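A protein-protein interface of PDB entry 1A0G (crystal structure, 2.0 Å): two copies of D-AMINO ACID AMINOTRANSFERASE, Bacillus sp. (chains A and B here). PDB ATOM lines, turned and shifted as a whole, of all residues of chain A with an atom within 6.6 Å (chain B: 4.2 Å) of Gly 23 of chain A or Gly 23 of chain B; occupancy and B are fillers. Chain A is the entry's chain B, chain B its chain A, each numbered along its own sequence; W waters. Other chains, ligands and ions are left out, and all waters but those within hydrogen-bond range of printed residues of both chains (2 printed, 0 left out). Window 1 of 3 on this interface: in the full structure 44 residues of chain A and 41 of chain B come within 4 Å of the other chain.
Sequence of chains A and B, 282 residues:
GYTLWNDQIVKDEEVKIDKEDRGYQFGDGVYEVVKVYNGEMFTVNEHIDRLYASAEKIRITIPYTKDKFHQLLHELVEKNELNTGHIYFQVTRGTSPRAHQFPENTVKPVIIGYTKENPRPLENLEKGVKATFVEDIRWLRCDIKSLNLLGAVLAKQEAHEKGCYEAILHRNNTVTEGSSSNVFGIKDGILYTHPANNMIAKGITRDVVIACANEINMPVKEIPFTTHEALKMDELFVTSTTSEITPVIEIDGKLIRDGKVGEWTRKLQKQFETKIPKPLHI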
ATOM      1  N   GLU A  20      25.310  -7.345  -6.598  1.00  0.00           N
ATOM      2  CA  GLU A  20      24.278  -7.772  -7.529  1.00  0.00           C
ATOM      3  C   GLU A  20      23.970  -6.714  -8.553  1.00  0.00           C
ATOM      4  O   GLU A  20      22.850  -6.604  -9.062  1.00  0.00           O
ATOM      5  CB  GLU A  20      23.018  -8.211  -6.800  1.00  0.00           C
ATOM      6  CG  GLU A  20      23.212  -9.483  -6.014  1.00  0.00           C
ATOM      7  CD  GLU A  20      21.919  -9.998  -5.450  1.00  0.00           C
ATOM      8  OE1 GLU A  20      21.339  -9.311  -4.592  1.00  0.00           O
ATOM      9  OE2 GLU A  20      21.490 -11.089  -5.859  1.00  0.00           O
ATOM     10  N   ASP A  21      24.960  -5.879  -8.801  1.00  0.00           N
ATOM     11  CA  ASP A  21      24.829  -4.861  -9.823  1.00  0.00           C
ATOM     12  C   ASP A  21      24.863  -5.751 -11.074  1.00  0.00           C
ATOM     13  O   ASP A  21      25.764  -6.584 -11.217  1.00  0.00           O
ATOM     14  CB  ASP A  21      26.056  -3.945  -9.768  1.00  0.00           C
ATOM     15  CG  ASP A  21      25.981  -2.795 -10.751  1.00  0.00           C
ATOM     16  OD1 ASP A  21      25.640  -3.032 -11.935  1.00  0.00           O
ATOM     17  OD2 ASP A  21      26.304  -1.663 -10.341  1.00  0.00           O
ATOM     18  N   ARG A  22      23.900  -5.582 -11.972  1.00  0.00           N
ATOM     19  CA  ARG A  22      23.842  -6.406 -13.173  1.00  0.00           C
ATOM     20  C   ARG A  22      25.070  -6.317 -14.075  1.00  0.00           C
ATOM     21  O   ARG A  22      25.339  -7.232 -14.852  1.00  0.00           O
ATOM     22  CB  ARG A  22      22.527  -6.163 -13.928  1.00  0.00           C
ATOM     23  CG  ARG A  22      21.321  -6.664 -13.114  1.00  0.00           C
ATOM     24  CD  ARG A  22      19.984  -6.373 -13.753  1.00  0.00           C
ATOM     25  NE  ARG A  22      19.855  -6.998 -15.062  1.00  0.00           N
ATOM     26  CZ  ARG A  22      19.190  -8.116 -15.312  1.00  0.00           C
ATOM     27  NH1 ARG A  22      18.569  -8.774 -14.338  1.00  0.00           N
ATOM     28  NH2 ARG A  22      19.152  -8.585 -16.549  1.00  0.00           N
ATOM     29  N   GLY A  23      25.837  -5.240 -13.932  1.00  0.00           N
ATOM     30  CA  GLY A  23      27.060  -5.064 -14.711  1.00  0.00           C
ATOM     31  C   GLY A  23      28.147  -5.974 -14.169  1.00  0.00           C
ATOM     32  O   GLY A  23      29.039  -6.397 -14.892  1.00  0.00           O
ATOM     33  N   TYR A  24      28.025  -6.322 -12.895  1.00  0.00           N
ATOM     34  CA  TYR A  24      28.973  -7.209 -12.245  1.00  0.00           C
ATOM     35  C   TYR A  24      28.616  -8.680 -12.464  1.00  0.00           C
ATOM     36  O   TYR A  24      29.499  -9.533 -12.511  1.00  0.00           O
ATOM     37  CB  TYR A  24      29.005  -6.924 -10.740  1.00  0.00           C
ATOM     38  CG  TYR A  24      30.210  -7.496 -10.027  1.00  0.00           C
ATOM     39  CD1 TYR A  24      31.490  -7.408 -10.592  1.00  0.00           C
ATOM     40  CD2 TYR A  24      30.083  -8.099  -8.779  1.00  0.00           C
ATOM     41  CE1 TYR A  24      32.602  -7.898  -9.913  1.00  0.00           C
ATOM     42  CE2 TYR A  24      31.185  -8.586  -8.104  1.00  0.00           C
ATOM     43  CZ  TYR A  24      32.435  -8.482  -8.668  1.00  0.00           C
ATOM     44  OH  TYR A  24      33.539  -8.926  -7.963  1.00  0.00           O
ATOM     45  N   GLN A  25      27.327  -8.977 -12.580  1.00  0.00           N
ATOM     46  CA  GLN A  25      26.882 -10.358 -12.748  1.00  0.00           C
ATOM     47  C   GLN A  25      26.587 -10.887 -14.155  1.00  0.00           C
ATOM     48  O   GLN A  25      26.708 -12.081 -14.384  1.00  0.00           O
ATOM     49  CB  GLN A  25      25.685 -10.633 -11.841  1.00  0.00           C
ATOM     50  CG  GLN A  25      26.007 -10.507 -10.362  1.00  0.00           C
ATOM     51  CD  GLN A  25      24.903 -11.045  -9.486  1.00  0.00           C
ATOM     52  OE1 GLN A  25      23.732 -10.742  -9.683  1.00  0.00           O
ATOM     53  NE2 GLN A  25      25.271 -11.836  -8.509  1.00  0.00           N
ATOM     54  N   PHE A  26      26.141 -10.012 -15.051  1.00  0.00           N
ATOM     55  CA  PHE A  26      25.810 -10.375 -16.434  1.00  0.00           C
ATOM     56  C   PHE A  26      26.517  -9.475 -17.460  1.00  0.00           C
ATOM     57  O   PHE A  26      26.281  -9.619 -18.668  1.00  0.00           O
ATOM     58  CB  PHE A  26      24.291 -10.235 -16.673  1.00  0.00           C
ATOM     59  CG  PHE A  26      23.421 -10.970 -15.658  1.00  0.00           C
ATOM     60  CD1 PHE A  26      23.268 -12.358 -15.713  1.00  0.00           C
ATOM     61  CD2 PHE A  26      22.765 -10.279 -14.656  1.00  0.00           C
ATOM     62  CE1 PHE A  26      22.471 -13.037 -14.776  1.00  0.00           C
ATOM     63  CE2 PHE A  26      21.971 -10.954 -13.717  1.00  0.00           C
ATOM     64  CZ  PHE A  26      21.831 -12.335 -13.785  1.00  0.00           C
ATOM     65  N   GLY A  27      27.352  -8.536 -17.000  1.00  0.00           N
ATOM     66  CA  GLY A  27      27.989  -7.598 -17.927  1.00  0.00           C
ATOM     67  C   GLY A  27      26.894  -6.809 -18.638  1.00  0.00           C
ATOM     68  O   GLY A  27      27.028  -6.391 -19.800  1.00  0.00           O
ATOM     69  N   ASP A  28      25.787  -6.627 -17.924  1.00  0.00           N
ATOM     70  CA  ASP A  28      24.594  -5.958 -18.434  1.00  0.00           C
ATOM     71  C   ASP A  28      24.709  -4.433 -18.398  1.00  0.00           C
ATOM     72  O   ASP A  28      24.142  -3.775 -17.528  1.00  0.00           O
ATOM     73  CB  ASP A  28      23.392  -6.433 -17.603  1.00  0.00           C
ATOM     74  CG  ASP A  28      22.058  -6.127 -18.239  1.00  0.00           C
ATOM     75  OD1 ASP A  28      22.006  -5.559 -19.343  1.00  0.00           O
ATOM     76  OD2 ASP A  28      21.037  -6.459 -17.608  1.00  0.00           O
ATOM     77  N   GLY A  29      25.397  -3.877 -19.383  1.00  0.00           N
ATOM     78  CA  GLY A  29      25.582  -2.444 -19.440  1.00  0.00           C
ATOM     79  C   GLY A  29      26.323  -2.044 -20.696  1.00  0.00           C
ATOM     80  O   GLY A  29      26.763  -2.907 -21.462  1.00  0.00           O
ATOM     81  N   GLN A  90      30.285   4.345 -17.971  1.00  0.00           N
ATOM     82  CA  GLN A  90      29.434   3.187 -18.262  1.00  0.00           C
ATOM     83  C   GLN A  90      28.093   3.274 -17.534  1.00  0.00           C
ATOM     84  O   GLN A  90      27.968   3.951 -16.516  1.00  0.00           O
ATOM     85  CB  GLN A  90      30.122   1.888 -17.846  1.00  0.00           C
ATOM     86  CG  GLN A  90      30.310   1.747 -16.348  1.00  0.00           C
ATOM     87  CD  GLN A  90      30.881   0.413 -15.944  1.00  0.00           C
ATOM     88  OE1 GLN A  90      32.001   0.077 -16.303  1.00  0.00           O
ATOM     89  NE2 GLN A  90      30.125  -0.346 -15.149  1.00  0.00           N
ATOM     90  N   THR A  92      24.858   0.524 -16.316  1.00  0.00           N
ATOM     91  CA  THR A  92      24.414  -0.856 -16.168  1.00  0.00           C
ATOM     92  C   THR A  92      22.933  -0.818 -15.826  1.00  0.00           C
ATOM     93  O   THR A  92      22.431   0.210 -15.366  1.00  0.00           O
ATOM     94  CB  THR A  92      25.149  -1.587 -15.049  1.00  0.00           C
ATOM     95  OG1 THR A  92      24.726  -1.082 -13.780  1.00  0.00           O
ATOM     96  CG2 THR A  92      26.648  -1.432 -15.179  1.00  0.00           C
ATOM     97  N   ARG A  93      22.230  -1.936 -16.005  1.00  0.00           N
ATOM     98  CA  ARG A  93      20.799  -1.968 -15.711  1.00  0.00           C
ATOM     99  C   ARG A  93      20.424  -1.591 -14.267  1.00  0.00           C
ATOM    100  O   ARG A  93      19.366  -1.008 -14.035  1.00  0.00           O
ATOM    101  CB  ARG A  93      20.191  -3.324 -16.093  1.00  0.00           C
ATOM    102  CG  ARG A  93      18.723  -3.221 -16.486  1.00  0.00           C
ATOM    103  CD  ARG A  93      18.148  -4.506 -17.098  1.00  0.00           C
ATOM    104  NE  ARG A  93      18.798  -4.854 -18.349  1.00  0.00           N
ATOM    105  CZ  ARG A  93      18.507  -4.333 -19.531  1.00  0.00           C
ATOM    106  NH1 ARG A  93      17.550  -3.425 -19.658  1.00  0.00           N
ATOM    107  NH2 ARG A  93      19.231  -4.682 -20.587  1.00  0.00           N
ATOM    108  N   GLY A  94      21.313  -1.854 -13.315  1.00  0.00           N
ATOM    109  CA  GLY A  94      21.019  -1.534 -11.931  1.00  0.00           C
ATOM    110  C   GLY A  94      21.267  -2.695 -10.994  1.00  0.00           C
ATOM    111  O   GLY A  94      21.791  -3.736 -11.411  1.00  0.00           O
ATOM    112  N   LEU A 147      29.318  -4.271 -21.948  1.00  0.00           N
ATOM    113  CA  LEU A 147      30.379  -4.712 -21.042  1.00  0.00           C
ATOM    114  C   LEU A 147      30.799  -6.175 -21.214  1.00  0.00           C
ATOM    115  O   LEU A 147      31.659  -6.679 -20.488  1.00  0.00           O
ATOM    116  CB  LEU A 147      29.988  -4.408 -19.587  1.00  0.00           C
ATOM    117  CG  LEU A 147      29.709  -2.920 -19.275  1.00  0.00           C
ATOM    118  CD1 LEU A 147      29.094  -2.758 -17.907  1.00  0.00           C
ATOM    119  CD2 LEU A 147      30.989  -2.092 -19.372  1.00  0.00           C
ATOM    120  N   ASP B  21      36.912  -3.357 -10.957  1.00  0.00           N
ATOM    121  CA  ASP B  21      37.011  -4.803 -10.840  1.00  0.00           C
ATOM    122  C   ASP B  21      36.766  -5.225 -12.298  1.00  0.00           C
ATOM    123  O   ASP B  21      35.798  -4.787 -12.920  1.00  0.00           O
ATOM    124  CB  ASP B  21      35.894  -5.340  -9.946  1.00  0.00           C
ATOM    125  CG  ASP B  21      36.026  -6.832  -9.653  1.00  0.00           C
ATOM    126  OD1 ASP B  21      36.269  -7.640 -10.587  1.00  0.00           O
ATOM    127  OD2 ASP B  21      35.847  -7.206  -8.474  1.00  0.00           O
ATOM    128  N   ARG B  22      37.638  -6.058 -12.849  1.00  0.00           N
ATOM    129  CA  ARG B  22      37.492  -6.498 -14.242  1.00  0.00           C
ATOM    130  C   ARG B  22      36.161  -7.221 -14.496  1.00  0.00           C
ATOM    131  O   ARG B  22      35.643  -7.205 -15.611  1.00  0.00           O
ATOM    132  CB  ARG B  22      38.697  -7.338 -14.657  1.00  0.00           C
ATOM    133  CG  ARG B  22      39.978  -6.512 -14.689  1.00  0.00           C
ATOM    134  CD  ARG B  22      41.195  -7.355 -14.997  1.00  0.00           C
ATOM    135  NE  ARG B  22      41.099  -7.961 -16.323  1.00  0.00           N
ATOM    136  CZ  ARG B  22      41.643  -7.465 -17.432  1.00  0.00           C
ATOM    137  NH1 ARG B  22      42.330  -6.334 -17.398  1.00  0.00           N
ATOM    138  NH2 ARG B  22      41.522  -8.120 -18.578  1.00  0.00           N
ATOM    139  N   GLY B  23      35.561  -7.769 -13.438  1.00  0.00           N
ATOM    140  CA  GLY B  23      34.285  -8.428 -13.600  1.00  0.00           C
ATOM    141  C   GLY B  23      33.233  -7.395 -13.913  1.00  0.00           C
ATOM    142  O   GLY B  23      32.279  -7.656 -14.655  1.00  0.00           O
ATOM    143  N   TYR B  24      33.447  -6.186 -13.418  1.00  0.00           N
ATOM    144  CA  TYR B  24      32.512  -5.087 -13.621  1.00  0.00           C
ATOM    145  C   TYR B  24      32.639  -4.363 -14.959  1.00  0.00           C
ATOM    146  O   TYR B  24      31.648  -3.897 -15.521  1.00  0.00           O
ATOM    147  CB  TYR B  24      32.715  -4.081 -12.501  1.00  0.00           C
ATOM    148  CG  TYR B  24      31.576  -3.134 -12.305  1.00  0.00           C
ATOM    149  CD1 TYR B  24      30.286  -3.606 -12.108  1.00  0.00           C
ATOM    150  CD2 TYR B  24      31.783  -1.761 -12.304  1.00  0.00           C
ATOM    151  CE1 TYR B  24      29.230  -2.731 -11.912  1.00  0.00           C
ATOM    152  CE2 TYR B  24      30.748  -0.882 -12.106  1.00  0.00           C
ATOM    153  CZ  TYR B  24      29.469  -1.367 -11.913  1.00  0.00           C
ATOM    154  OH  TYR B  24      28.430  -0.479 -11.744  1.00  0.00           O
ATOM    155  N   GLN B  25      33.868  -4.222 -15.437  1.00  0.00           N
ATOM    156  CA  GLN B  25      34.144  -3.526 -16.682  1.00  0.00           C
ATOM    157  C   GLN B  25      34.231  -4.411 -17.921  1.00  0.00           C
ATOM    158  O   GLN B  25      34.017  -3.921 -19.021  1.00  0.00           O
ATOM    159  CB  GLN B  25      35.445  -2.720 -16.565  1.00  0.00           C
ATOM    160  CG  GLN B  25      35.460  -1.738 -15.417  1.00  0.00           C
ATOM    161  CD  GLN B  25      36.594  -0.750 -15.511  1.00  0.00           C
ATOM    162  OE1 GLN B  25      37.757  -1.130 -15.578  1.00  0.00           O
ATOM    163  NE2 GLN B  25      36.262   0.525 -15.504  1.00  0.00           N
ATOM    164  N   GLY B  27      33.229  -8.138 -17.681  1.00  0.00           N
ATOM    165  CA  GLY B  27      32.554  -9.405 -17.468  1.00  0.00           C
ATOM    166  C   GLY B  27      33.626 -10.477 -17.354  1.00  0.00           C
ATOM    167  O   GLY B  27      33.363 -11.674 -17.549  1.00  0.00           O
ATOM    168  N   ASP B  28      34.822 -10.053 -16.953  1.00  0.00           N
ATOM    169  CA  ASP B  28      35.982 -10.931 -16.853  1.00  0.00           C
ATOM    170  C   ASP B  28      36.034 -11.829 -15.617  1.00  0.00           C
ATOM    171  O   ASP B  28      36.851 -11.629 -14.698  1.00  0.00           O
ATOM    172  CB  ASP B  28      37.251 -10.084 -16.974  1.00  0.00           C
ATOM    173  CG  ASP B  28      38.500 -10.908 -17.163  1.00  0.00           C
ATOM    174  OD1 ASP B  28      38.434 -12.160 -17.244  1.00  0.00           O
ATOM    175  OD2 ASP B  28      39.575 -10.284 -17.262  1.00  0.00           O
ATOM    176  N   THR B  92      36.511 -13.153 -10.277  1.00  0.00           N
ATOM    177  CA  THR B  92      36.889 -12.240 -11.348  1.00  0.00           C
ATOM    178  C   THR B  92      38.406 -12.171 -11.327  1.00  0.00           C
ATOM    179  O   THR B  92      39.016 -12.520 -10.319  1.00  0.00           O
ATOM    180  CB  THR B  92      36.281 -10.832 -11.190  1.00  0.00           C
ATOM    181  OG1 THR B  92      36.824 -10.167 -10.038  1.00  0.00           O
ATOM    182  CG2 THR B  92      34.768 -10.914 -11.079  1.00  0.00           C
HETATM  183  O   HOH W   1      33.712   1.132 -14.170  1.00  0.00           O
HETATM  184  O   HOH W   2      28.063   1.408 -13.985  1.00  0.00           O
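Of the 8 printed residues of chain B, 6 touch a printed residue of chain A. Printed residues of chain B that touch a printed residue of chain A: Asp 21, Gly 23, Tyr 24, Gln 25, Gly 27 and Thr 92. Hydrophobic or aromatic side chains of chain B within 4 Å of the printed part of chain A: Tyr 24. Of the 15 printed residues of chain A, 6 touch a printed residue of chain B. Among the printed residues, 12 pairs touch across the chains. Among the printed residues, no Asp or Glu carboxylate lies within 4 Å of a Lys or Arg side-chain nitrogen of the other chain.
Gly 23 of chain A touches just these residues of chain B: Gly 23 (3.5 Å) and Tyr 24 (3.7 Å). Printed residues of chain B within 4 Å of Tyr 24 of chain A: Asp 21 (2.9 Å), Gly 23 (3.8 Å), Tyr 24 (3.6 Å) and Thr 92 (3.9 Å). Printed residues of chain A within 4 Å of Gly 23 of chain B: Gly 23 (3.5 Å) and Tyr 24 (3.8 Å). Printed residues of chain A within 4 Å of Tyr 24 of chain B: Asp 21 (2.8 Å), Gly 23 (3.7 Å), Tyr 24 (3.6 Å), Gln 90 (3.2 Å), Thr 92 (3.99 Å) and Leu 147 (3.7 Å). The nearest residue of chain A that does not touch Gly 23 of chain B is Gly 27 of chain A (5.4 Å).
The side-chain hydroxyl of Tyr 24 of chain A sits at hydrogen-bond distance from the side-chain carboxylate of Asp 21 of chain B, at 2.9 Å. The backbone carbonyl oxygen of Gly 23 of chain B lies close to the backbone carbonyl oxygen of Gly 23 of chain A (3.5 Å). The side-chain carboxylate (OD2) of Asp 21 of chain A is in hydrogen-bond range of the side-chain hydroxyl (OH) of Tyr 24 of chain B.
Asp 21 of chain A touches Tyr 24 of chain B, and with the chains exchanged Tyr 24 of chain A touches Asp 21 of chain B. Gly 23 of chain B touches its own counterpart, Gly 23 of chain A. Gly 23 of chain A touches Tyr 24 of chain B, and with the chains exchanged Tyr 24 of chain A touches Gly 23 of chain B. Tyr 24 of chain A touches Thr 92 of chain B, and with the chains exchanged Thr 92 of chain A touches Tyr 24 of chain B. Positions printed for both chains: 21, 22, 23, 24, 25, 27, 28 and 92.
Water W1 lies within hydrogen-bond range of the side-chain amide oxygen (OE1) of Gln 90 of chain A (2.9 Å) and the side-chain amide nitrogen (NE2) of Gln 25 of chain B (2.9 Å). Water W2 lies within hydrogen-bond range of NE2 of Gln 90 of chain A (2.9 Å) and OH of Tyr 24 of chain B (3.0 Å).
O of Gly 23 of chain A touches O of Tyr 24 of chain B, at 3.7 Å. CD1 of Tyr 24 of chain A touches C of Gly 23 of chain B, at 3.8 Å. Tyr 24 of chain B touches Tyr 24 of chain A. CG2 of Thr 92 of chain B touches CE1 of Tyr 24 of chain A, 3.9 Å away. Tyr 24 of chain B touches Gln 90 of chain A (CE2 to NE2, 3.2 Å). Tyr 24 of chain B touches Thr 92 of chain A (OH to CG2, 3.99 Å). CD1 of Leu 147 of chain A touches O of Tyr 24 of chain B, 3.7 Å away. O of Gln 25 of chain B touches CD2 of Leu 147 of chain A, at 3.6 Å. O of Leu 147 of chain A touches N of Gly 27 of chain B (3.5 Å).
The side-chain carboxylate (OD1) of Asp 21 of chain A is in hydrogen-bond range of the backbone NH (N) of Gly 23 of chain A, 3.0 Å away. The side-chain carboxylate of Asp 21 of chain B is in hydrogen-bond range of the side-chain hydroxyl of Thr 92 of chain B (2.6 Å). The side-chain carboxylate (OD1) of Asp 21 of chain B lies within hydrogen-bond range of the backbone NH (N) of Gly 23 of chain B. The side-chain carboxylate (OD1) of Asp 21 of chain A sits at hydrogen-bond distance from the side-chain hydroxyl (OG1) of Thr 92 of chain A, at 2.8 Å. O of Gly 29 of chain A lies within hydrogen-bond range of N of Leu 147 of chain A (2.9 Å). O of Arg 22 of chain B is in hydrogen-bond range of N of Gly 27 of chain B, at 3.3 Å.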
